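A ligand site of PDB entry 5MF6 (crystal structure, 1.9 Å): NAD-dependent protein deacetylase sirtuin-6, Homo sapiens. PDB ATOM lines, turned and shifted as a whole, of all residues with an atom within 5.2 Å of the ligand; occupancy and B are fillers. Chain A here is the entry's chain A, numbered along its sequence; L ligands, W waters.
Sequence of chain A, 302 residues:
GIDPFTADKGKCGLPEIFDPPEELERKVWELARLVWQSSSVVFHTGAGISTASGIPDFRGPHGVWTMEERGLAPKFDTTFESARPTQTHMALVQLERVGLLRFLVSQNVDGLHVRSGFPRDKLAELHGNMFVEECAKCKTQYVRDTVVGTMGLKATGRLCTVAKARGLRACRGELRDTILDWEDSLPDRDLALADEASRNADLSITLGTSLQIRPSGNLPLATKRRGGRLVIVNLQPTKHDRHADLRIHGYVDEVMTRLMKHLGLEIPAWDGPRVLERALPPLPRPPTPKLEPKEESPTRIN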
ATOM      1  N   GLU A  16      -6.555  -2.482  17.414  1.00  0.00           N
ATOM      2  CA  GLU A  16      -5.335  -2.505  18.286  1.00  0.00           C
ATOM      3  C   GLU A  16      -5.714  -3.253  19.551  1.00  0.00           C
ATOM      4  O   GLU A  16      -6.873  -3.251  19.956  1.00  0.00           O
ATOM      5  CB  GLU A  16      -4.850  -1.152  18.624  1.00  0.00           C
ATOM      6  CG  GLU A  16      -4.326  -0.423  17.420  1.00  0.00           C
ATOM      7  CD  GLU A  16      -3.823   0.963  17.759  1.00  0.00           C
ATOM      8  OE1 GLU A  16      -4.376   1.661  18.575  1.00  0.00           O
ATOM      9  OE2 GLU A  16      -2.871   1.391  17.106  1.00  0.00           O
ATOM     10  N   THR A  45      12.384  -5.346  12.485  1.00  0.00           N
ATOM     11  CA  THR A  45      11.605  -4.145  12.741  1.00  0.00           C
ATOM     12  C   THR A  45      10.766  -3.729  11.491  1.00  0.00           C
ATOM     13  O   THR A  45      11.207  -3.905  10.342  1.00  0.00           O
ATOM     14  CB  THR A  45      12.488  -2.899  13.091  1.00  0.00           C
ATOM     15  OG1 THR A  45      13.421  -2.699  12.071  1.00  0.00           O
ATOM     16  CG2 THR A  45      13.201  -3.111  14.453  1.00  0.00           C
ATOM     17  N   GLY A  46       9.633  -3.130  11.743  1.00  0.00           N
ATOM     18  CA  GLY A  46       8.841  -2.466  10.705  1.00  0.00           C
ATOM     19  C   GLY A  46       8.390  -1.144  11.141  1.00  0.00           C
ATOM     20  O   GLY A  46       8.944  -0.472  12.058  1.00  0.00           O
ATOM     21  N   ALA A  47       7.359  -0.666  10.447  1.00  0.00           N
ATOM     22  CA  ALA A  47       7.026   0.732  10.382  1.00  0.00           C
ATOM     23  C   ALA A  47       6.573   1.269  11.660  1.00  0.00           C
ATOM     24  O   ALA A  47       6.628   2.479  12.020  1.00  0.00           O
ATOM     25  CB  ALA A  47       6.024   0.943   9.223  1.00  0.00           C
ATOM     26  N   GLY A  48       6.079   0.348  12.478  1.00  0.00           N
ATOM     27  CA  GLY A  48       5.610   0.665  13.778  1.00  0.00           C
ATOM     28  C   GLY A  48       6.648   1.238  14.767  1.00  0.00           C
ATOM     29  O   GLY A  48       6.301   1.998  15.624  1.00  0.00           O
ATOM     30  N   THR A  51       6.500   5.308  14.162  1.00  0.00           N
ATOM     31  CA  THR A  51       5.357   6.087  14.413  1.00  0.00           C
ATOM     32  C   THR A  51       5.529   7.129  15.491  1.00  0.00           C
ATOM     33  O   THR A  51       4.958   8.233  15.394  1.00  0.00           O
ATOM     34  CB  THR A  51       4.085   5.153  14.625  1.00  0.00           C
ATOM     35  OG1 THR A  51       4.288   4.291  15.753  1.00  0.00           O
ATOM     36  CG2 THR A  51       3.764   4.338  13.416  1.00  0.00           C
ATOM     37  N   ALA A  52       6.291   6.833  16.583  1.00  0.00           N
ATOM     38  CA  ALA A  52       6.564   7.782  17.670  1.00  0.00           C
ATOM     39  C   ALA A  52       7.530   8.923  17.330  1.00  0.00           C
ATOM     40  O   ALA A  52       7.676   9.832  18.158  1.00  0.00           O
ATOM     41  CB  ALA A  52       7.025   7.094  18.971  1.00  0.00           C
ATOM     42  N   ASP A  57       2.691   4.527   9.875  1.00  0.00           N
ATOM     43  CA  ASP A  57       2.931   3.195   9.359  1.00  0.00           C
ATOM     44  C   ASP A  57       2.097   2.929   8.072  1.00  0.00           C
ATOM     45  O   ASP A  57       1.614   3.946   7.535  1.00  0.00           O
ATOM     46  CB  ASP A  57       2.804   2.171  10.525  1.00  0.00           C
ATOM     47  CG  ASP A  57       1.364   2.027  11.047  1.00  0.00           C
ATOM     48  OD1 ASP A  57       0.410   2.364  10.306  1.00  0.00           O
ATOM     49  OD2 ASP A  57       1.191   1.603  12.192  1.00  0.00           O
ATOM     50  N   PHE A  58       1.951   1.648   7.665  1.00  0.00           N
ATOM     51  CA  PHE A  58       1.264   1.247   6.455  1.00  0.00           C
ATOM     52  C   PHE A  58      -0.160   0.751   6.767  1.00  0.00           C
ATOM     53  O   PHE A  58      -1.081   1.091   6.041  1.00  0.00           O
ATOM     54  CB  PHE A  58       2.003   0.257   5.650  1.00  0.00           C
ATOM     55  CG  PHE A  58       3.289   0.850   5.066  1.00  0.00           C
ATOM     56  CD1 PHE A  58       3.233   1.607   3.865  1.00  0.00           C
ATOM     57  CD2 PHE A  58       4.496   0.722   5.749  1.00  0.00           C
ATOM     58  CE1 PHE A  58       4.384   2.186   3.343  1.00  0.00           C
ATOM     59  CE2 PHE A  58       5.668   1.324   5.209  1.00  0.00           C
ATOM     60  CZ  PHE A  58       5.574   2.093   4.040  1.00  0.00           C
ATOM     61  N   ARG A  59      -0.289  -0.071   7.835  1.00  0.00           N
ATOM     62  CA  ARG A  59      -1.523  -0.900   8.071  1.00  0.00           C
ATOM     63  C   ARG A  59      -2.138  -0.663   9.445  1.00  0.00           C
ATOM     64  O   ARG A  59      -3.208  -1.222   9.772  1.00  0.00           O
ATOM     65  CB  ARG A  59      -1.264  -2.362   7.799  1.00  0.00           C
ATOM     66  CG  ARG A  59      -0.791  -2.698   6.402  1.00  0.00           C
ATOM     67  CD  ARG A  59      -0.516  -4.084   6.071  1.00  0.00           C
ATOM     68  NE  ARG A  59       0.087  -4.309   4.781  1.00  0.00           N
ATOM     69  CZ  ARG A  59       1.361  -4.012   4.451  1.00  0.00           C
ATOM     70  NH1 ARG A  59       2.222  -3.628   5.413  1.00  0.00           N
ATOM     71  NH2 ARG A  59       1.867  -4.169   3.244  1.00  0.00           N
ATOM     72  N   GLY A  60      -1.603   0.286  10.205  1.00  0.00           N
ATOM     73  CA  GLY A  60      -2.186   0.761  11.418  1.00  0.00           C
ATOM     74  C   GLY A  60      -3.489   1.505  11.184  1.00  0.00           C
ATOM     75  O   GLY A  60      -3.858   1.735  10.008  1.00  0.00           O
ATOM     76  N   TRP A  65      -1.732   2.724   3.813  1.00  0.00           N
ATOM     77  CA  TRP A  65      -2.694   1.929   3.103  1.00  0.00           C
ATOM     78  C   TRP A  65      -4.082   1.968   3.750  1.00  0.00           C
ATOM     79  O   TRP A  65      -5.137   2.102   3.044  1.00  0.00           O
ATOM     80  CB  TRP A  65      -2.196   0.503   2.856  1.00  0.00           C
ATOM     81  CG  TRP A  65      -0.826   0.280   2.288  1.00  0.00           C
ATOM     82  CD1 TRP A  65      -0.025  -0.771   2.617  1.00  0.00           C
ATOM     83  CD2 TRP A  65      -0.122   1.025   1.300  1.00  0.00           C
ATOM     84  NE1 TRP A  65       1.134  -0.733   1.922  1.00  0.00           N
ATOM     85  CE2 TRP A  65       1.121   0.365   1.109  1.00  0.00           C
ATOM     86  CE3 TRP A  65      -0.406   2.208   0.566  1.00  0.00           C
ATOM     87  CZ2 TRP A  65       2.074   0.812   0.214  1.00  0.00           C
ATOM     88  CZ3 TRP A  65       0.560   2.698  -0.309  1.00  0.00           C
ATOM     89  CH2 TRP A  65       1.807   2.035  -0.455  1.00  0.00           C
ATOM     90  N   GLN A 107      12.359  -3.783   7.558  1.00  0.00           N
ATOM     91  CA  GLN A 107      11.556  -3.454   6.414  1.00  0.00           C
ATOM     92  C   GLN A 107      11.451  -1.994   6.167  1.00  0.00           C
ATOM     93  O   GLN A 107      10.894  -1.610   5.154  1.00  0.00           O
ATOM     94  CB  GLN A 107      10.161  -4.112   6.623  1.00  0.00           C
ATOM     95  CG  GLN A 107      10.240  -5.614   6.602  1.00  0.00           C
ATOM     96  CD  GLN A 107       8.953  -6.242   7.033  1.00  0.00           C
ATOM     97  OE1 GLN A 107       7.988  -6.209   6.251  1.00  0.00           O
ATOM     98  NE2 GLN A 107       8.868  -6.650   8.338  1.00  0.00           N
ATOM     99  N   ASN A 108      11.981  -1.117   7.043  1.00  0.00           N
ATOM    100  CA  ASN A 108      11.766   0.235   6.913  1.00  0.00           C
ATOM    101  C   ASN A 108      12.710   0.872   5.879  1.00  0.00           C
ATOM    102  O   ASN A 108      13.971   0.556   5.822  1.00  0.00           O
ATOM    103  CB  ASN A 108      11.919   0.970   8.203  1.00  0.00           C
ATOM    104  CG  ASN A 108      10.977   0.423   9.242  1.00  0.00           C
ATOM    105  OD1 ASN A 108      10.009  -0.257   8.876  1.00  0.00           O
ATOM    106  ND2 ASN A 108      11.285   0.647  10.497  1.00  0.00           N
ATOM    107  N   HIS A 127      13.885  -3.545   2.170  1.00  0.00           N
ATOM    108  CA  HIS A 127      12.998  -2.838   1.213  1.00  0.00           C
ATOM    109  C   HIS A 127      13.685  -1.599   0.674  1.00  0.00           C
ATOM    110  O   HIS A 127      13.108  -0.901  -0.151  1.00  0.00           O
ATOM    111  CB  HIS A 127      11.676  -2.542   1.891  1.00  0.00           C
ATOM    112  CG  HIS A 127      10.928  -3.790   2.242  1.00  0.00           C
ATOM    113  ND1 HIS A 127       9.814  -3.794   3.062  1.00  0.00           N
ATOM    114  CD2 HIS A 127      11.191  -5.077   1.949  1.00  0.00           C
ATOM    115  CE1 HIS A 127       9.421  -5.034   3.241  1.00  0.00           C
ATOM    116  NE2 HIS A 127      10.208  -5.834   2.566  1.00  0.00           N
ATOM    117  N   TRP A 182       6.780  -2.830  -5.948  1.00  0.00           N
ATOM    118  CA  TRP A 182       6.103  -4.130  -5.807  1.00  0.00           C
ATOM    119  C   TRP A 182       6.732  -5.324  -6.563  1.00  0.00           C
ATOM    120  O   TRP A 182       6.908  -6.365  -5.963  1.00  0.00           O
ATOM    121  CB  TRP A 182       4.608  -3.974  -6.199  1.00  0.00           C
ATOM    122  CG  TRP A 182       3.893  -3.129  -5.197  1.00  0.00           C
ATOM    123  CD1 TRP A 182       3.523  -1.824  -5.339  1.00  0.00           C
ATOM    124  CD2 TRP A 182       3.491  -3.522  -3.875  1.00  0.00           C
ATOM    125  NE1 TRP A 182       2.896  -1.377  -4.188  1.00  0.00           N
ATOM    126  CE2 TRP A 182       2.879  -2.400  -3.263  1.00  0.00           C
ATOM    127  CE3 TRP A 182       3.593  -4.719  -3.125  1.00  0.00           C
ATOM    128  CZ2 TRP A 182       2.373  -2.418  -1.941  1.00  0.00           C
ATOM    129  CZ3 TRP A 182       3.070  -4.748  -1.816  1.00  0.00           C
ATOM    130  CH2 TRP A 182       2.478  -3.602  -1.244  1.00  0.00           C
ATOM    131  N   GLY A 208       6.948  -3.827  15.911  1.00  0.00           N
ATOM    132  CA  GLY A 208       6.236  -2.882  14.987  1.00  0.00           C
ATOM    133  C   GLY A 208       6.158  -3.281  13.518  1.00  0.00           C
ATOM    134  O   GLY A 208       6.319  -2.438  12.621  1.00  0.00           O
ATOM    135  N   THR A 209       5.983  -4.576  13.292  1.00  0.00           N
ATOM    136  CA  THR A 209       5.628  -5.189  12.019  1.00  0.00           C
ATOM    137  C   THR A 209       4.393  -6.118  12.138  1.00  0.00           C
ATOM    138  O   THR A 209       4.303  -6.900  13.048  1.00  0.00           O
ATOM    139  CB  THR A 209       6.780  -5.872  11.316  1.00  0.00           C
ATOM    140  OG1 THR A 209       6.425  -6.393  10.024  1.00  0.00           O
ATOM    141  CG2 THR A 209       7.494  -6.971  12.126  1.00  0.00           C
ATOM    142  N   SER A 210       3.492  -5.984  11.165  1.00  0.00           N
ATOM    143  CA  SER A 210       2.325  -6.896  11.031  1.00  0.00           C
ATOM    144  C   SER A 210       2.675  -8.194  10.355  1.00  0.00           C
ATOM    145  O   SER A 210       1.803  -9.110  10.301  1.00  0.00           O
ATOM    146  CB  SER A 210       1.134  -6.129  10.365  1.00  0.00           C
ATOM    147  OG  SER A 210       1.421  -5.915   9.000  1.00  0.00           O
ATOM    148  N   LEU A 211       3.904  -8.355   9.797  1.00  0.00           N
ATOM    149  CA  LEU A 211       4.480  -9.581   9.232  1.00  0.00           C
ATOM    150  C   LEU A 211       3.768 -10.166   7.972  1.00  0.00           C
ATOM    151  O   LEU A 211       3.844 -11.365   7.696  1.00  0.00           O
ATOM    152  CB  LEU A 211       4.722 -10.716  10.272  1.00  0.00           C
ATOM    153  CG  LEU A 211       5.515 -10.277  11.530  1.00  0.00           C
ATOM    154  CD1 LEU A 211       5.369 -11.310  12.661  1.00  0.00           C
ATOM    155  CD2 LEU A 211       7.002 -10.129  11.103  1.00  0.00           C
ATOM    156  N   GLN A 212       3.142  -9.265   7.235  1.00  0.00           N
ATOM    157  CA  GLN A 212       2.328  -9.675   6.086  1.00  0.00           C
ATOM    158  C   GLN A 212       3.083  -9.804   4.777  1.00  0.00           C
ATOM    159  O   GLN A 212       2.535 -10.353   3.820  1.00  0.00           O
ATOM    160  CB  GLN A 212       1.180  -8.689   5.978  1.00  0.00           C
ATOM    161  CG  GLN A 212       0.269  -8.617   7.161  1.00  0.00           C
ATOM    162  CD  GLN A 212      -1.029  -7.864   6.918  1.00  0.00           C
ATOM    163  OE1 GLN A 212      -1.759  -8.174   5.956  1.00  0.00           O
ATOM    164  NE2 GLN A 212      -1.349  -6.909   7.759  1.00  0.00           N
ATOM    165  N   ILE A 213       4.300  -9.205   4.665  1.00  0.00           N
ATOM    166  CA  ILE A 213       5.054  -9.212   3.403  1.00  0.00           C
ATOM    167  C   ILE A 213       5.964 -10.380   3.436  1.00  0.00           C
ATOM    168  O   ILE A 213       6.553 -10.692   4.444  1.00  0.00           O
ATOM    169  CB  ILE A 213       5.932  -7.938   3.242  1.00  0.00           C
ATOM    170  CG1 ILE A 213       5.034  -6.746   3.003  1.00  0.00           C
ATOM    171  CG2 ILE A 213       6.969  -8.082   2.108  1.00  0.00           C
ATOM    172  CD1 ILE A 213       4.285  -6.776   1.681  1.00  0.00           C
ATOM    173  N   VAL A 233       6.161  -8.084  19.215  1.00  0.00           N
ATOM    174  CA  VAL A 233       5.755  -6.933  20.005  1.00  0.00           C
ATOM    175  C   VAL A 233       5.029  -6.118  18.890  1.00  0.00           C
ATOM    176  O   VAL A 233       5.648  -5.724  17.917  1.00  0.00           O
ATOM    177  CB  VAL A 233       6.915  -6.077  20.590  1.00  0.00           C
ATOM    178  CG1 VAL A 233       6.405  -4.857  21.310  1.00  0.00           C
ATOM    179  CG2 VAL A 233       7.851  -6.957  21.526  1.00  0.00           C
ATOM    180  N   ASN A 234       3.758  -5.853  19.136  1.00  0.00           N
ATOM    181  CA  ASN A 234       2.834  -5.192  18.129  1.00  0.00           C
ATOM    182  C   ASN A 234       1.487  -4.825  18.748  1.00  0.00           C
ATOM    183  O   ASN A 234       0.951  -5.591  19.561  1.00  0.00           O
ATOM    184  CB  ASN A 234       2.670  -6.036  16.875  1.00  0.00           C
ATOM    185  CG  ASN A 234       2.473  -5.178  15.611  1.00  0.00           C
ATOM    186  OD1 ASN A 234       3.324  -4.352  15.270  1.00  0.00           O
ATOM    187  ND2 ASN A 234       1.310  -5.321  14.948  1.00  0.00           N
ATOM    188  N   LEU A 235       0.955  -3.641  18.421  1.00  0.00           N
ATOM    189  CA  LEU A 235      -0.373  -3.176  18.826  1.00  0.00           C
ATOM    190  C   LEU A 235      -1.505  -3.939  18.130  1.00  0.00           C
ATOM    191  O   LEU A 235      -2.492  -4.248  18.780  1.00  0.00           O
ATOM    192  CB  LEU A 235      -0.554  -1.699  18.566  1.00  0.00           C
ATOM    193  CG  LEU A 235       0.247  -0.819  19.547  1.00  0.00           C
ATOM    194  CD1 LEU A 235       0.146   0.610  19.076  1.00  0.00           C
ATOM    195  CD2 LEU A 235      -0.326  -0.989  20.947  1.00  0.00           C
ATOM    196  N   GLN A 236      -1.310  -4.327  16.903  1.00  0.00           N
ATOM    197  CA  GLN A 236      -2.398  -5.028  16.132  1.00  0.00           C
ATOM    198  C   GLN A 236      -1.985  -6.498  16.201  1.00  0.00           C
ATOM    199  O   GLN A 236      -0.791  -6.839  16.355  1.00  0.00           O
ATOM    200  CB  GLN A 236      -2.397  -4.598  14.710  1.00  0.00           C
ATOM    201  CG  GLN A 236      -3.037  -3.296  14.462  1.00  0.00           C
ATOM    202  CD  GLN A 236      -2.937  -2.843  12.998  1.00  0.00           C
ATOM    203  OE1 GLN A 236      -1.948  -3.103  12.245  1.00  0.00           O
ATOM    204  NE2 GLN A 236      -3.997  -2.093  12.580  1.00  0.00           N
ATOM    205  N   PRO A 237      -2.907  -7.390  15.829  1.00  0.00           N
ATOM    206  CA  PRO A 237      -2.548  -8.708  15.366  1.00  0.00           C
ATOM    207  C   PRO A 237      -1.579  -8.734  14.227  1.00  0.00           C
ATOM    208  O   PRO A 237      -1.536  -7.843  13.445  1.00  0.00           O
ATOM    209  CB  PRO A 237      -3.899  -9.345  14.851  1.00  0.00           C
ATOM    210  CG  PRO A 237      -4.917  -8.429  15.369  1.00  0.00           C
ATOM    211  CD  PRO A 237      -4.332  -7.062  15.586  1.00  0.00           C
ATOM    212  N   GLY A 250       1.491  -3.654  23.178  1.00  0.00           N
ATOM    213  CA  GLY A 250       1.772  -2.378  23.803  1.00  0.00           C
ATOM    214  C   GLY A 250       2.639  -1.498  22.947  1.00  0.00           C
ATOM    215  O   GLY A 250       3.056  -1.918  21.845  1.00  0.00           O
ATOM    216  N   TYR A 251       2.855  -0.289  23.386  1.00  0.00           N
ATOM    217  CA  TYR A 251       3.696   0.604  22.570  1.00  0.00           C
ATOM    218  C   TYR A 251       5.138   0.133  22.640  1.00  0.00           C
ATOM    219  O   TYR A 251       5.632  -0.108  23.781  1.00  0.00           O
ATOM    220  CB  TYR A 251       3.544   2.024  23.036  1.00  0.00           C
ATOM    221  CG  TYR A 251       2.194   2.604  22.747  1.00  0.00           C
ATOM    222  CD1 TYR A 251       1.862   3.095  21.470  1.00  0.00           C
ATOM    223  CD2 TYR A 251       1.266   2.693  23.752  1.00  0.00           C
ATOM    224  CE1 TYR A 251       0.622   3.689  21.284  1.00  0.00           C
ATOM    225  CE2 TYR A 251      -0.008   3.146  23.521  1.00  0.00           C
ATOM    226  CZ  TYR A 251      -0.322   3.674  22.295  1.00  0.00           C
ATOM    227  OH  TYR A 251      -1.594   4.156  22.188  1.00  0.00           O
ATOM    228  N   VAL A 252       5.835   0.046  21.471  1.00  0.00           N
ATOM    229  CA  VAL A 252       7.169  -0.490  21.419  1.00  0.00           C
ATOM    230  C   VAL A 252       8.147   0.353  22.236  1.00  0.00           C
ATOM    231  O   VAL A 252       8.924  -0.238  22.984  1.00  0.00           O
ATOM    232  CB  VAL A 252       7.823  -0.758  20.075  1.00  0.00           C
ATOM    233  CG1 VAL A 252       7.248  -1.985  19.383  1.00  0.00           C
ATOM    234  CG2 VAL A 252       7.753   0.467  19.126  1.00  0.00           C
ATOM    235  N   ASP A 253       7.939   1.644  22.321  1.00  0.00           N
ATOM    236  CA  ASP A 253       8.843   2.482  23.172  1.00  0.00           C
ATOM    237  C   ASP A 253       8.686   2.125  24.651  1.00  0.00           C
ATOM    238  O   ASP A 253       9.717   2.133  25.363  1.00  0.00           O
ATOM    239  CB  ASP A 253       8.659   3.948  22.978  1.00  0.00           C
ATOM    240  CG  ASP A 253       9.381   4.514  21.723  1.00  0.00           C
ATOM    241  OD1 ASP A 253      10.160   3.824  21.054  1.00  0.00           O
ATOM    242  OD2 ASP A 253       9.044   5.663  21.383  1.00  0.00           O
HETATM  243  N1  LIG L   1       4.183   0.286  19.112  1.00  0.00           N
HETATM  244  C1  LIG L   1       3.818  -0.971  18.790  1.00  0.00           C
HETATM  245  N2  LIG L   1       3.304  -1.337  17.604  1.00  0.00           N
HETATM  246  C2  LIG L   1       3.058  -0.266  16.757  1.00  0.00           C
HETATM  247  C3  LIG L   1       3.313   1.099  17.045  1.00  0.00           C
HETATM  248  C4  LIG L   1       3.985   1.376  18.307  1.00  0.00           C
HETATM  249  N3  LIG L   1       4.273   2.661  18.706  1.00  0.00           N
HETATM  250  N4  LIG L   1       2.989   1.844  15.949  1.00  0.00           N
HETATM  251  C5  LIG L   1       2.477   0.974  15.059  1.00  0.00           C
HETATM  252  N5  LIG L   1       2.494  -0.280  15.527  1.00  0.00           N
HETATM  253  P1  LIG L   1       2.651  -2.330   8.863  1.00  0.00           P
HETATM  254  P2  LIG L   1       5.258  -3.318   8.082  1.00  0.00           P
HETATM  255  C6  LIG L   1       2.164  -1.531  14.837  1.00  0.00           C
HETATM  256  O1  LIG L   1       2.188  -3.525   8.032  1.00  0.00           O
HETATM  257  O2  LIG L   1       6.627  -2.700   8.328  1.00  0.00           O
HETATM  258  C7  LIG L   1       4.559  -1.991   3.191  1.00  0.00           C
HETATM  259  O3  LIG L   1       3.923  -2.161   1.895  1.00  0.00           O
HETATM  260  C8  LIG L   1       0.806  -1.516  14.018  1.00  0.00           C
HETATM  261  O4  LIG L   1      -0.241  -1.906  14.904  1.00  0.00           O
HETATM  262  O5  LIG L   1       2.111  -0.968   8.990  1.00  0.00           O
HETATM  263  O6  LIG L   1       5.043  -4.727   8.657  1.00  0.00           O
HETATM  264  C9  LIG L   1       6.036  -1.445   3.095  1.00  0.00           C
HETATM  265  O7  LIG L   1       6.709  -2.051   1.993  1.00  0.00           O
HETATM  266  C10 LIG L   1       1.088  -2.357  12.835  1.00  0.00           C
HETATM  267  O8  LIG L   1       0.647  -3.704  12.787  1.00  0.00           O
HETATM  268  O9  LIG L   1       4.257  -2.153   8.450  1.00  0.00           O
HETATM  269  C11 LIG L   1       6.690  -2.052   4.367  1.00  0.00           C
HETATM  270  O10 LIG L   1       8.156  -2.163   4.374  1.00  0.00           O
HETATM  271  C12 LIG L   1       2.687  -2.432  12.747  1.00  0.00           C
HETATM  272  O11 LIG L   1       3.096  -1.627  13.826  1.00  0.00           O
HETATM  273  C13 LIG L   1       6.059  -3.465   4.331  1.00  0.00           C
HETATM  274  O12 LIG L   1       4.751  -3.300   3.751  1.00  0.00           O
HETATM  275  C14 LIG L   1       3.238  -2.023  11.421  1.00  0.00           C
HETATM  276  O13 LIG L   1       2.689  -2.856  10.385  1.00  0.00           O
HETATM  277  C15 LIG L   1       5.803  -4.182   5.682  1.00  0.00           C
HETATM  278  O14 LIG L   1       5.044  -3.285   6.513  1.00  0.00           O
HETATM  279  O   HOH W   1       8.466  -0.400   1.257  1.00  0.00           O
HETATM  280  O   HOH W   2      -0.376   2.453  14.018  1.00  0.00           O
HETATM  281  O   HOH W   3      -1.442   0.382  15.450  1.00  0.00           O
HETATM  282  O   HOH W   4       3.504  -6.356   7.219  1.00  0.00           O
HETATM  283  O   HOH W   5       8.264  -1.006   6.898  1.00  0.00           O
HETATM  284  O   HOH W   6       9.216   0.544   4.144  1.00  0.00           O
HETATM  285  O   HOH W   7       6.435   3.454  20.537  1.00  0.00           O
HETATM  286  O   HOH W   8       7.054   4.055  17.508  1.00  0.00           O
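The side-chain hydroxyl (OG1) of Thr 209 lies within hydrogen-bond range of the side-chain amide nitrogen (NE2) of Gln 107. The backbone carbonyl oxygen (O) of Gln 236 sits at hydrogen-bond distance from the side-chain amide nitrogen (ND2) of Asn 234 (2.9 Å). The backbone carbonyl oxygen of Gly 48 is in hydrogen-bond range of the side-chain hydroxyl of Thr 51 (3.1 Å). O of Thr 45 is in hydrogen-bond range of N of Gln 107, at 3.0 Å. The backbone carbonyl oxygen (O) of Phe 58 is in hydrogen-bond range of the backbone NH (N) of Trp 65 (2.8 Å). ND2 of Asn 108 is in hydrogen-bond range of O of Gly 46 (3.0 Å). The backbone carbonyl oxygen (O) of Gly 208 lies within hydrogen-bond range of the backbone NH (N) of Gly 48, 2.8 Å away. The backbone NH of Gly 208 is in hydrogen-bond range of the backbone carbonyl oxygen of Val 233 (3.1 Å).
The backbone carbonyl oxygen (O) of Gly 48 sits close to a nitrogen (N4) of the ligand (3.3 Å). CA of Gly 46 touches O2 of the ligand, 3.3 Å away. OD2 of Asp 57 touches C5 of the ligand, 3.2 Å away. Trp 182 touches the ligand (CH2 to O3, 3.7 Å). Gly 208 touches the ligand (O to C14, 3.3 Å). Leu 211 touches the ligand. CG1 of Ile 213 touches O12 of the ligand (3.5 Å). Gly 250 touches the ligand (O to C1, 3.3 Å). Tyr 251 touches the ligand (CA to N1, 3.5 Å). Hydrophobic or aromatic side chains within 4 Å of the ligand: Ala 47, Phe 58, Trp 65, His 127, Trp 182, Ile 213, Leu 235, Tyr 251 and Val 252. Within 4 Å of the ligand: Gly 46, Ala 47, Gly 48, Thr 51, Asp 57, Phe 58, Arg 59, Trp 65, Gln 107, His 127, Trp 182, Gly 208, Thr 209, Ser 210, Leu 211, Ile 213, Asn 234, Leu 235, Gln 236, Gly 250, Tyr 251 and Val 252.
Water W3 bridges the side-chain carboxylate (OE2) of Glu 16 (2.4 Å) and an oxygen (O4) of the ligand (2.6 Å). Water W4 lies within hydrogen-bond range of O6 of the ligand, OG of Ser 210, N of Gln 212 and N of Leu 211. Water W5 lies within hydrogen-bond range of the side-chain amide oxygen (OD1) of Asn 108 (2.7 Å), an oxygen (O2) of the ligand (2.8 Å) and the backbone carbonyl oxygen (O) of Gln 107 (3.2 Å). Water W6 bridges the backbone carbonyl oxygen of Gln 107 (2.9 Å) and an oxygen (O10) of the ligand (2.9 Å). Water W7 lies within hydrogen-bond range of N3 of the ligand (2.9 Å) and N of Asp 253 (3.0 Å). Water W8 lies within hydrogen-bond range of O of Gly 48, N of Ala 52, OG1 of Thr 51 and N3 of the ligand.
An oxygen (O6) of the ligand lies within hydrogen-bond range of the side-chain hydroxyl (OG1) of Thr 209 (2.6 Å). The backbone NH (N) of Arg 59 lies within hydrogen-bond range of an oxygen (O5) of the ligand. The guanidinium group of Arg 59 is in salt-bridge range of an oxygen (O1) of the ligand, 2.6 Å away. A ring nitrogen (ND1) of His 127 is in hydrogen-bond range of an oxygen (O10) of the ligand (2.7 Å). O6 of the ligand is in hydrogen-bond range of N of Ser 210. OG of Ser 210 sits at hydrogen-bond distance from O1 of the ligand. An oxygen (O4) of the ligand lies close to the backbone NH of Gln 236 (3.3 Å). The side-chain amide oxygen (OE1) of Gln 236 is in hydrogen-bond range of an oxygen (O8) of the ligand (2.7 Å). OG1 of Thr 51 sits at hydrogen-bond distance from N4 of the ligand (2.8 Å). ND2 of Asn 234 lies within hydrogen-bond range of O8 of the ligand. N1 of the ligand is in hydrogen-bond range of N of Val 252, at 2.9 Å. An oxygen (O10) of the ligand sits at hydrogen-bond distance from the backbone carbonyl oxygen of Gln 107. N of Phe 58 lies within hydrogen-bond range of O5 of the ligand (2.9 Å). N of Ala 47 sits at hydrogen-bond distance from O2 of the ligand (3.0 Å). NE1 of Trp 65 sits at hydrogen-bond distance from O3 of the ligand. N of Leu 235 is in hydrogen-bond range of N2 of the ligand.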
